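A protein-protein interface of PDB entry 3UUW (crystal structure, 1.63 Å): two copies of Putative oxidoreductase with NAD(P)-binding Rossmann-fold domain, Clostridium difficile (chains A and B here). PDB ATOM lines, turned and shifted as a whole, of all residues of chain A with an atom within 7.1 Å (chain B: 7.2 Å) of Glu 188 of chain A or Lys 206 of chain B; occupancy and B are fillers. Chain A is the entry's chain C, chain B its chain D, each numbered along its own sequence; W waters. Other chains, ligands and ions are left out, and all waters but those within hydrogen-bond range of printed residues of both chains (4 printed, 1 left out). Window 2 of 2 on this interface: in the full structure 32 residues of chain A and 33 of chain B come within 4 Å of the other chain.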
ATOM      1  N   ILE A 185      23.548 -24.368 -10.478  1.00  0.00           N
ATOM      2  CA  ILE A 185      22.906 -24.404 -11.791  1.00  0.00           C
ATOM      3  C   ILE A 185      22.796 -22.975 -12.300  1.00  0.00           C
ATOM      4  O   ILE A 185      22.169 -22.126 -11.642  1.00  0.00           O
ATOM      5  CB  ILE A 185      21.521 -25.050 -11.724  1.00  0.00           C
ATOM      6  CG1 ILE A 185      21.666 -26.533 -11.370  1.00  0.00           C
ATOM      7  CG2 ILE A 185      20.797 -24.924 -13.064  1.00  0.00           C
ATOM      8  CD1 ILE A 185      20.342 -27.198 -11.032  1.00  0.00           C
ATOM      9  N   SER A 186      23.423 -22.700 -13.446  1.00  0.00           N
ATOM     10  CA  SER A 186      23.426 -21.353 -14.029  1.00  0.00           C
ATOM     11  C   SER A 186      22.657 -21.295 -15.342  1.00  0.00           C
ATOM     12  O   SER A 186      22.559 -20.232 -15.969  1.00  0.00           O
ATOM     13  CB  SER A 186      24.861 -20.861 -14.238  1.00  0.00           C
ATOM     14  OG  SER A 186      25.555 -21.691 -15.157  1.00  0.00           O
ATOM     15  N   GLY A 187      22.100 -22.430 -15.751  1.00  0.00           N
ATOM     16  CA  GLY A 187      21.285 -22.514 -16.957  1.00  0.00           C
ATOM     17  C   GLY A 187      20.635 -23.883 -17.031  1.00  0.00           C
ATOM     18  O   GLY A 187      21.166 -24.862 -16.488  1.00  0.00           O
ATOM     19  N   GLU A 188      19.482 -23.940 -17.685  1.00  0.00           N
ATOM     20  CA  GLU A 188      18.696 -25.157 -17.802  1.00  0.00           C
ATOM     21  C   GLU A 188      17.775 -25.116 -19.011  1.00  0.00           C
ATOM     22  O   GLU A 188      17.128 -24.112 -19.257  1.00  0.00           O
ATOM     23  CB  GLU A 188      17.807 -25.364 -16.562  1.00  0.00           C
ATOM     24  CG  GLU A 188      16.751 -26.471 -16.736  1.00  0.00           C
ATOM     25  CD  GLU A 188      15.943 -26.732 -15.465  1.00  0.00           C
ATOM     26  OE1 GLU A 188      16.457 -27.412 -14.544  1.00  0.00           O
ATOM     27  OE2 GLU A 188      14.786 -26.259 -15.409  1.00  0.00           O
ATOM     28  N   ASP A 189      17.752 -26.223 -19.758  1.00  0.00           N
ATOM     29  CA  ASP A 189      16.726 -26.490 -20.769  1.00  0.00           C
ATOM     30  C   ASP A 189      16.056 -27.801 -20.383  1.00  0.00           C
ATOM     31  O   ASP A 189      16.721 -28.751 -19.994  1.00  0.00           O
ATOM     32  CB  ASP A 189      17.308 -26.693 -22.168  1.00  0.00           C
ATOM     33  CG  ASP A 189      18.151 -25.545 -22.638  1.00  0.00           C
ATOM     34  OD1 ASP A 189      17.693 -24.389 -22.547  1.00  0.00           O
ATOM     35  OD2 ASP A 189      19.293 -25.820 -23.116  1.00  0.00           O
ATOM     36  N   LEU A 190      14.736 -27.863 -20.510  1.00  0.00           N
ATOM     37  CA  LEU A 190      14.006 -29.091 -20.277  1.00  0.00           C
ATOM     38  C   LEU A 190      12.840 -29.143 -21.240  1.00  0.00           C
ATOM     39  O   LEU A 190      11.892 -28.359 -21.100  1.00  0.00           O
ATOM     40  CB  LEU A 190      13.518 -29.202 -18.835  1.00  0.00           C
ATOM     41  CG  LEU A 190      12.769 -30.505 -18.493  1.00  0.00           C
ATOM     42  CD1 LEU A 190      13.604 -31.798 -18.703  1.00  0.00           C
ATOM     43  CD2 LEU A 190      12.241 -30.457 -17.068  1.00  0.00           C
ATOM     44  N   PHE A 191      12.905 -30.059 -22.205  1.00  0.00           N
ATOM     45  CA  PHE A 191      11.863 -30.196 -23.225  1.00  0.00           C
ATOM     46  C   PHE A 191      11.204 -31.561 -23.096  1.00  0.00           C
ATOM     47  O   PHE A 191      11.890 -32.598 -23.118  1.00  0.00           O
ATOM     48  CB  PHE A 191      12.440 -30.004 -24.643  1.00  0.00           C
ATOM     49  CG  PHE A 191      13.243 -28.729 -24.811  1.00  0.00           C
ATOM     50  CD1 PHE A 191      12.888 -27.564 -24.134  1.00  0.00           C
ATOM     51  CD2 PHE A 191      14.338 -28.692 -25.675  1.00  0.00           C
ATOM     52  CE1 PHE A 191      13.617 -26.393 -24.289  1.00  0.00           C
ATOM     53  CE2 PHE A 191      15.069 -27.536 -25.849  1.00  0.00           C
ATOM     54  CZ  PHE A 191      14.719 -26.372 -25.137  1.00  0.00           C
ATOM     55  N   VAL A 201      17.279 -32.528 -22.154  1.00  0.00           N
ATOM     56  CA  VAL A 201      17.607 -31.815 -20.955  1.00  0.00           C
ATOM     57  C   VAL A 201      19.035 -31.327 -21.054  1.00  0.00           C
ATOM     58  O   VAL A 201      19.917 -32.016 -21.611  1.00  0.00           O
ATOM     59  CB  VAL A 201      17.380 -32.667 -19.685  1.00  0.00           C
ATOM     60  CG1 VAL A 201      18.181 -33.972 -19.730  1.00  0.00           C
ATOM     61  CG2 VAL A 201      17.686 -31.844 -18.426  1.00  0.00           C
ATOM     62  N   SER A 202      19.260 -30.126 -20.553  1.00  0.00           N
ATOM     63  CA  SER A 202      20.619 -29.608 -20.444  1.00  0.00           C
ATOM     64  C   SER A 202      20.769 -28.677 -19.269  1.00  0.00           C
ATOM     65  O   SER A 202      19.821 -28.029 -18.869  1.00  0.00           O
ATOM     66  CB  SER A 202      21.070 -28.891 -21.716  1.00  0.00           C
ATOM     67  OG  SER A 202      20.414 -27.659 -21.853  1.00  0.00           O
ATOM     68  N   HIS A 203      21.980 -28.639 -18.717  1.00  0.00           N
ATOM     69  CA  HIS A 203      22.306 -27.720 -17.643  1.00  0.00           C
ATOM     70  C   HIS A 203      23.686 -27.108 -17.793  1.00  0.00           C
ATOM     71  O   HIS A 203      24.563 -27.675 -18.450  1.00  0.00           O
ATOM     72  CB  HIS A 203      22.222 -28.395 -16.275  1.00  0.00           C
ATOM     73  CG  HIS A 203      20.834 -28.758 -15.894  1.00  0.00           C
ATOM     74  ND1 HIS A 203      20.277 -29.970 -16.231  1.00  0.00           N
ATOM     75  CD2 HIS A 203      19.860 -28.041 -15.290  1.00  0.00           C
ATOM     76  CE1 HIS A 203      19.017 -29.994 -15.822  1.00  0.00           C
ATOM     77  NE2 HIS A 203      18.738 -28.833 -15.253  1.00  0.00           N
ATOM     78  N   LYS A 204      23.853 -25.930 -17.194  1.00  0.00           N
ATOM     79  CA  LYS A 204      25.189 -25.352 -17.032  1.00  0.00           C
ATOM     80  C   LYS A 204      25.412 -25.357 -15.521  1.00  0.00           C
ATOM     81  O   LYS A 204      24.579 -24.854 -14.757  1.00  0.00           O
ATOM     82  CB  LYS A 204      25.316 -23.964 -17.678  1.00  0.00           C
ATOM     83  CG  LYS A 204      26.743 -23.339 -17.545  1.00  0.00           C
ATOM     84  CD  LYS A 204      26.908 -21.983 -18.300  1.00  0.00           C
ATOM     85  CE  LYS A 204      27.490 -22.177 -19.731  1.00  0.00           C
ATOM     86  NZ  LYS A 204      27.946 -20.894 -20.437  1.00  0.00           N
ATOM     87  N   LYS A 302      16.284 -31.477  -6.913  1.00  0.00           N
ATOM     88  CA  LYS A 302      16.091 -30.030  -6.905  1.00  0.00           C
ATOM     89  C   LYS A 302      15.596 -29.559  -8.280  1.00  0.00           C
ATOM     90  O   LYS A 302      14.720 -28.698  -8.374  1.00  0.00           O
ATOM     91  CB  LYS A 302      17.400 -29.344  -6.493  1.00  0.00           C
ATOM     92  CG  LYS A 302      17.336 -27.840  -6.326  1.00  0.00           C
ATOM     93  CD  LYS A 302      18.687 -27.313  -5.831  1.00  0.00           C
ATOM     94  CE  LYS A 302      18.862 -25.822  -6.101  1.00  0.00           C
ATOM     95  NZ  LYS A 302      17.843 -24.989  -5.450  1.00  0.00           N
ATOM     96  N   ILE A 303      16.149 -30.143  -9.346  1.00  0.00           N
ATOM     97  CA  ILE A 303      15.724 -29.845 -10.693  1.00  0.00           C
ATOM     98  C   ILE A 303      14.261 -30.252 -10.907  1.00  0.00           C
ATOM     99  O   ILE A 303      13.447 -29.460 -11.365  1.00  0.00           O
ATOM    100  CB  ILE A 303      16.670 -30.550 -11.700  1.00  0.00           C
ATOM    101  CG1 ILE A 303      18.047 -29.875 -11.662  1.00  0.00           C
ATOM    102  CG2 ILE A 303      16.073 -30.554 -13.110  1.00  0.00           C
ATOM    103  CD1 ILE A 303      19.177 -30.691 -12.336  1.00  0.00           C
ATOM    104  N   ILE A 304      13.932 -31.480 -10.520  1.00  0.00           N
ATOM    105  CA  ILE A 304      12.592 -32.027 -10.683  1.00  0.00           C
ATOM    106  C   ILE A 304      11.573 -31.186  -9.908  1.00  0.00           C
ATOM    107  O   ILE A 304      10.503 -30.853 -10.429  1.00  0.00           O
ATOM    108  CB  ILE A 304      12.569 -33.504 -10.240  1.00  0.00           C
ATOM    109  CG1 ILE A 304      13.366 -34.344 -11.247  1.00  0.00           C
ATOM    110  CG2 ILE A 304      11.132 -34.033 -10.132  1.00  0.00           C
ATOM    111  CD1 ILE A 304      13.756 -35.728 -10.746  1.00  0.00           C
ATOM    112  N   SER A 306      11.782 -28.082  -9.122  1.00  0.00           N
ATOM    113  CA  SER A 306      11.687 -26.710  -9.651  1.00  0.00           C
ATOM    114  C   SER A 306      10.765 -26.590 -10.880  1.00  0.00           C
ATOM    115  O   SER A 306      10.381 -25.480 -11.260  1.00  0.00           O
ATOM    116  CB  SER A 306      13.080 -26.172 -10.008  1.00  0.00           C
ATOM    117  OG  SER A 306      13.596 -26.797 -11.182  1.00  0.00           O
ATOM    118  N   VAL A 307      10.411 -27.720 -11.494  1.00  0.00           N
ATOM    119  CA  VAL A 307       9.579 -27.728 -12.709  1.00  0.00           C
ATOM    120  C   VAL A 307       8.143 -27.302 -12.410  1.00  0.00           C
ATOM    121  O   VAL A 307       7.454 -27.935 -11.612  1.00  0.00           O
ATOM    122  CB  VAL A 307       9.579 -29.135 -13.386  1.00  0.00           C
ATOM    123  CG1 VAL A 307       8.787 -29.126 -14.698  1.00  0.00           C
ATOM    124  CG2 VAL A 307      10.990 -29.588 -13.641  1.00  0.00           C
ATOM    125  N   GLU B 181      15.207 -16.122 -33.897  1.00  0.00           N
ATOM    126  CA  GLU B 181      14.197 -15.842 -32.872  1.00  0.00           C
ATOM    127  C   GLU B 181      14.917 -15.072 -31.773  1.00  0.00           C
ATOM    128  O   GLU B 181      16.142 -15.180 -31.642  1.00  0.00           O
ATOM    129  CB  GLU B 181      13.548 -17.121 -32.305  1.00  0.00           C
ATOM    130  CG  GLU B 181      14.457 -18.025 -31.434  1.00  0.00           C
ATOM    131  CD  GLU B 181      13.687 -19.146 -30.713  1.00  0.00           C
ATOM    132  OE1 GLU B 181      12.450 -19.039 -30.583  1.00  0.00           O
ATOM    133  OE2 GLU B 181      14.322 -20.127 -30.252  1.00  0.00           O
ATOM    134  N   ASP B 182      14.164 -14.297 -30.995  1.00  0.00           N
ATOM    135  CA  ASP B 182      14.729 -13.512 -29.895  1.00  0.00           C
ATOM    136  C   ASP B 182      15.422 -14.439 -28.906  1.00  0.00           C
ATOM    137  O   ASP B 182      14.946 -15.553 -28.662  1.00  0.00           O
ATOM    138  CB  ASP B 182      13.629 -12.760 -29.125  1.00  0.00           C
ATOM    139  CG  ASP B 182      12.716 -11.952 -30.027  1.00  0.00           C
ATOM    140  OD1 ASP B 182      13.044 -11.775 -31.218  1.00  0.00           O
ATOM    141  OD2 ASP B 182      11.657 -11.502 -29.540  1.00  0.00           O
ATOM    142  N   VAL B 183      16.530 -13.979 -28.330  1.00  0.00           N
ATOM    143  CA  VAL B 183      17.228 -14.740 -27.290  1.00  0.00           C
ATOM    144  C   VAL B 183      17.629 -13.853 -26.125  1.00  0.00           C
ATOM    145  O   VAL B 183      17.777 -12.633 -26.262  1.00  0.00           O
ATOM    146  CB  VAL B 183      18.518 -15.451 -27.804  1.00  0.00           C
ATOM    147  CG1 VAL B 183      18.188 -16.444 -28.894  1.00  0.00           C
ATOM    148  CG2 VAL B 183      19.540 -14.433 -28.285  1.00  0.00           C
ATOM    149  N   GLU B 184      17.778 -14.478 -24.966  1.00  0.00           N
ATOM    150  CA  GLU B 184      18.242 -13.804 -23.769  1.00  0.00           C
ATOM    151  C   GLU B 184      19.512 -14.482 -23.280  1.00  0.00           C
ATOM    152  O   GLU B 184      19.622 -15.711 -23.304  1.00  0.00           O
ATOM    153  CB  GLU B 184      17.177 -13.848 -22.669  1.00  0.00           C
ATOM    154  CG  GLU B 184      15.890 -13.107 -23.034  1.00  0.00           C
ATOM    155  CD  GLU B 184      14.979 -12.840 -21.835  1.00  0.00           C
ATOM    156  OE1 GLU B 184      15.488 -12.458 -20.759  1.00  0.00           O
ATOM    157  OE2 GLU B 184      13.744 -12.987 -21.977  1.00  0.00           O
ATOM    158  N   ILE B 185      20.491 -13.632 -22.974  1.00  0.00           N
ATOM    159  CA  ILE B 185      21.799 -14.042 -22.523  1.00  0.00           C
ATOM    160  C   ILE B 185      21.748 -14.462 -21.084  1.00  0.00           C
ATOM    161  O   ILE B 185      21.008 -13.890 -20.273  1.00  0.00           O
ATOM    162  CB  ILE B 185      22.793 -12.877 -22.561  1.00  0.00           C
ATOM    163  CG1 ILE B 185      22.858 -12.239 -23.936  1.00  0.00           C
ATOM    164  CG2 ILE B 185      24.175 -13.342 -22.146  1.00  0.00           C
ATOM    165  CD1 ILE B 185      23.766 -11.039 -23.937  1.00  0.00           C
ATOM    166  N   SER B 186      22.579 -15.437 -20.761  1.00  0.00           N
ATOM    167  CA  SER B 186      22.678 -15.951 -19.417  1.00  0.00           C
ATOM    168  C   SER B 186      23.869 -16.878 -19.379  1.00  0.00           C
ATOM    169  O   SER B 186      24.533 -17.093 -20.402  1.00  0.00           O
ATOM    170  CB  SER B 186      21.413 -16.725 -19.052  1.00  0.00           C
ATOM    171  OG  SER B 186      20.291 -15.865 -19.002  1.00  0.00           O
ATOM    172  N   HIS B 203      28.709 -18.251 -23.309  1.00  0.00           N
ATOM    173  CA  HIS B 203      27.370 -17.820 -22.969  1.00  0.00           C
ATOM    174  C   HIS B 203      26.343 -18.855 -23.355  1.00  0.00           C
ATOM    175  O   HIS B 203      26.610 -19.742 -24.155  1.00  0.00           O
ATOM    176  CB  HIS B 203      27.010 -16.512 -23.672  1.00  0.00           C
ATOM    177  CG  HIS B 203      27.788 -15.351 -23.174  1.00  0.00           C
ATOM    178  ND1 HIS B 203      29.006 -14.998 -23.702  1.00  0.00           N
ATOM    179  CD2 HIS B 203      27.546 -14.482 -22.162  1.00  0.00           C
ATOM    180  CE1 HIS B 203      29.482 -13.961 -23.040  1.00  0.00           C
ATOM    181  NE2 HIS B 203      28.617 -13.628 -22.099  1.00  0.00           N
ATOM    182  N   LYS B 204      25.194 -18.756 -22.724  1.00  0.00           N
ATOM    183  CA  LYS B 204      24.050 -19.509 -23.145  1.00  0.00           C
ATOM    184  C   LYS B 204      23.025 -18.483 -23.608  1.00  0.00           C
ATOM    185  O   LYS B 204      22.635 -17.580 -22.833  1.00  0.00           O
ATOM    186  CB  LYS B 204      23.504 -20.365 -22.014  1.00  0.00           C
ATOM    187  CG  LYS B 204      22.353 -21.222 -22.452  1.00  0.00           C
ATOM    188  CD  LYS B 204      21.832 -22.067 -21.320  1.00  0.00           C
ATOM    189  CE  LYS B 204      20.755 -22.990 -21.809  1.00  0.00           C
ATOM    190  NZ  LYS B 204      19.926 -23.458 -20.658  1.00  0.00           N
ATOM    191  N   LEU B 205      22.576 -18.605 -24.855  1.00  0.00           N
ATOM    192  CA  LEU B 205      21.592 -17.698 -25.408  1.00  0.00           C
ATOM    193  C   LEU B 205      20.282 -18.468 -25.496  1.00  0.00           C
ATOM    194  O   LEU B 205      20.137 -19.383 -26.312  1.00  0.00           O
ATOM    195  CB  LEU B 205      22.033 -17.157 -26.777  1.00  0.00           C
ATOM    196  CG  LEU B 205      23.433 -16.526 -26.843  1.00  0.00           C
ATOM    197  CD1 LEU B 205      23.671 -16.012 -28.246  1.00  0.00           C
ATOM    198  CD2 LEU B 205      23.628 -15.409 -25.807  1.00  0.00           C
ATOM    199  N   LYS B 206      19.333 -18.113 -24.633  1.00  0.00           N
ATOM    200  CA  LYS B 206      18.092 -18.872 -24.539  1.00  0.00           C
ATOM    201  C   LYS B 206      16.935 -18.288 -25.344  1.00  0.00           C
ATOM    202  O   LYS B 206      16.516 -17.141 -25.130  1.00  0.00           O
ATOM    203  CB  LYS B 206      17.693 -19.041 -23.068  1.00  0.00           C
ATOM    204  CG  LYS B 206      16.545 -20.037 -22.849  1.00  0.00           C
ATOM    205  CD  LYS B 206      16.565 -20.614 -21.424  1.00  0.00           C
ATOM    206  CE  LYS B 206      15.418 -21.607 -21.156  1.00  0.00           C
ATOM    207  NZ  LYS B 206      15.558 -22.921 -21.865  1.00  0.00           N
ATOM    208  N   GLY B 207      16.417 -19.095 -26.265  1.00  0.00           N
ATOM    209  CA  GLY B 207      15.245 -18.743 -27.065  1.00  0.00           C
ATOM    210  C   GLY B 207      14.039 -19.518 -26.567  1.00  0.00           C
ATOM    211  O   GLY B 207      14.156 -20.382 -25.703  1.00  0.00           O
ATOM    212  N   LYS B 208      12.877 -19.218 -27.124  1.00  0.00           N
ATOM    213  CA  LYS B 208      11.648 -19.889 -26.747  1.00  0.00           C
ATOM    214  C   LYS B 208      11.689 -21.398 -27.059  1.00  0.00           C
ATOM    215  O   LYS B 208      11.190 -22.208 -26.274  1.00  0.00           O
ATOM    216  CB  LYS B 208      10.473 -19.206 -27.461  1.00  0.00           C
ATOM    217  CG  LYS B 208       9.128 -19.890 -27.341  1.00  0.00           C
ATOM    218  CD  LYS B 208       8.050 -19.101 -28.094  1.00  0.00           C
ATOM    219  CE  LYS B 208       6.768 -19.910 -28.263  1.00  0.00           C
ATOM    220  NZ  LYS B 208       6.989 -21.128 -29.105  1.00  0.00           N
ATOM    221  N   ASN B 209      12.294 -21.772 -28.183  1.00  0.00           N
ATOM    222  CA  ASN B 209      12.323 -23.177 -28.625  1.00  0.00           C
ATOM    223  C   ASN B 209      13.636 -23.944 -28.397  1.00  0.00           C
ATOM    224  O   ASN B 209      13.653 -25.180 -28.384  1.00  0.00           O
ATOM    225  CB  ASN B 209      11.929 -23.258 -30.108  1.00  0.00           C
ATOM    226  CG  ASN B 209      10.498 -22.798 -30.365  1.00  0.00           C
ATOM    227  OD1 ASN B 209      10.256 -21.998 -31.261  1.00  0.00           O
ATOM    228  ND2 ASN B 209       9.555 -23.293 -29.576  1.00  0.00           N
ATOM    229  N   PHE B 210      14.738 -23.225 -28.245  1.00  0.00           N
ATOM    230  CA  PHE B 210      16.013 -23.853 -27.941  1.00  0.00           C
ATOM    231  C   PHE B 210      17.018 -22.796 -27.557  1.00  0.00           C
ATOM    232  O   PHE B 210      16.786 -21.586 -27.719  1.00  0.00           O
ATOM    233  CB  PHE B 210      16.558 -24.674 -29.116  1.00  0.00           C
ATOM    234  CG  PHE B 210      16.772 -23.881 -30.384  1.00  0.00           C
ATOM    235  CD1 PHE B 210      15.768 -23.795 -31.330  1.00  0.00           C
ATOM    236  CD2 PHE B 210      17.971 -23.248 -30.637  1.00  0.00           C
ATOM    237  CE1 PHE B 210      15.958 -23.081 -32.499  1.00  0.00           C
ATOM    238  CE2 PHE B 210      18.165 -22.539 -31.811  1.00  0.00           C
ATOM    239  CZ  PHE B 210      17.156 -22.458 -32.730  1.00  0.00           C
ATOM    240  N   SER B 211      18.142 -23.275 -27.070  1.00  0.00           N
ATOM    241  CA  SER B 211      19.242 -22.411 -26.677  1.00  0.00           C
ATOM    242  C   SER B 211      20.480 -22.651 -27.529  1.00  0.00           C
ATOM    243  O   SER B 211      20.650 -23.714 -28.172  1.00  0.00           O
ATOM    244  CB  SER B 211      19.580 -22.642 -25.217  1.00  0.00           C
ATOM    245  OG  SER B 211      18.438 -22.409 -24.405  1.00  0.00           O
ATOM    246  N   ILE B 212      21.337 -21.641 -27.542  1.00  0.00           N
ATOM    247  CA  ILE B 212      22.604 -21.711 -28.238  1.00  0.00           C
ATOM    248  C   ILE B 212      23.719 -21.490 -27.238  1.00  0.00           C
ATOM    249  O   ILE B 212      23.729 -20.493 -26.531  1.00  0.00           O
ATOM    250  CB  ILE B 212      22.739 -20.674 -29.377  1.00  0.00           C
ATOM    251  CG1 ILE B 212      21.544 -20.765 -30.347  1.00  0.00           C
ATOM    252  CG2 ILE B 212      24.059 -20.869 -30.107  1.00  0.00           C
ATOM    253  CD1 ILE B 212      20.448 -19.824 -30.033  1.00  0.00           C
HETATM  254  O   HOH W   1      18.904 -21.199 -18.827  1.00  0.00           O
HETATM  255  O   HOH W   2      13.544 -25.160 -20.898  1.00  0.00           O
HETATM  256  O   HOH W   3      21.785 -25.523 -20.313  1.00  0.00           O
HETATM  257  O   HOH W   4      18.650 -25.962 -25.965  1.00  0.00           O
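Of chain B, only Lys 204 and Lys 206 come within 4 Å of Glu 188 of chain A. Of the printed residues of chain B, Asp 189 of chain A touches Lys 204 (3.1 Å), Lys 206 (2.7 Å) and Ser 211 (2.8 Å). Ser 306 of chain A touches none of the printed residues of chain B. Printed residues of chain A within 4 Å of His 203 of chain B: Lys 204 (3.9 Å). Printed residues of chain A within 4 Å of Ser 211 of chain B: Asp 189 (2.8 Å). The nearest residue of chain B that does not touch Glu 188 of chain A is Ser 211 of chain B (5.6 Å). The nearest printed residue of chain A that does not touch Ser 211 of chain B is Phe 191 of chain A (5.0 Å).
Water W3 lies within hydrogen-bond range of NZ of Lys 204 of chain B (2.8 Å) and OG of Ser 202 of chain A (3.0 Å). Water W4 bridges OD2 of Asp 189 of chain A and N of Ser 211 of chain B. Water W2 lies within hydrogen-bond range of the backbone NH of Leu 190 of chain A (3.0 Å) and the side-chain amino group of Lys 206 of chain B (3.2 Å). Water W1 lies within hydrogen-bond range of N of Glu 188 of chain A (3.0 Å) and NZ of Lys 204 of chain B (3.1 Å).
Of the 16 printed residues of chain A, 5 touch a printed residue of chain B. Hydrophobic or aromatic side chains of chain A that line the printed part of chain B: Phe 191. Among the printed residues, Asp or Glu carboxylates within 4 Å of a Lys or Arg side-chain nitrogen of the other chain: Asp 189 of chain A with Lys 204 of chain B and Asp 189 of chain A with Lys 206 of chain B.
Among the printed residues, merely in contact across the chains: Phe 191 of chain A with Asn 209 of chain B (3.6 Å), Gly 187 of chain A with Lys 204 of chain B (3.7 Å), Lys 204 of chain A with His 203 of chain B (3.9 Å) and Phe 191 of chain A with Phe 210 of chain B (3.99 Å).
Lys 204 of chain A touches His 203 of chain B, but with the chains exchanged His 203 of chain A does not touch Lys 204 of chain B (5.7 Å). Positions printed for both chains: 185, 186, 203 and 204. Of the 9 pairs that touch across the chains among the printed residues, none has its exchanged pair printed and touching as well.
The backbone carbonyl oxygen (O) of Glu 188 of chain A sits at hydrogen-bond distance from the side-chain amino group (NZ) of Lys 206 of chain B (3.3 Å). O of Glu 188 of chain A sits close to NZ of Lys 204 of chain B (3.2 Å). OD1 of Asp 189 of chain A is in salt-bridge range of NZ of Lys 206 of chain B. The side-chain carboxylate (OD1) of Asp 189 of chain A lies within salt-bridge range of the side-chain amino group (NZ) of Lys 204 of chain B (3.1 Å). OG of Ser 211 of chain B is in hydrogen-bond range of OD1 of Asp 189 of chain A (2.8 Å).
The side-chain carboxylate (OD2) of Asp 189 of chain A sits at hydrogen-bond distance from the side-chain hydroxyl (OG) of Ser 202 of chain A (2.5 Å). The backbone carbonyl oxygen (O) of Gly 187 of chain A sits at hydrogen-bond distance from the backbone NH (N) of Lys 204 of chain A, at 3.0 Å. The backbone carbonyl oxygen (O) of Ser 186 of chain B lies within hydrogen-bond range of the backbone NH (N) of Lys 204 of chain B. The side-chain carboxylate of Glu 181 of chain B is in hydrogen-bond range of the backbone NH of Asn 209 of chain B (3.3 Å). NZ of Lys 208 of chain B sits close to ND2 of Asn 209 of chain B (3.4 Å). The backbone carbonyl oxygen (O) of Glu 184 of chain B sits at hydrogen-bond distance from the backbone NH (N) of Lys 206 of chain B (2.8 Å).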
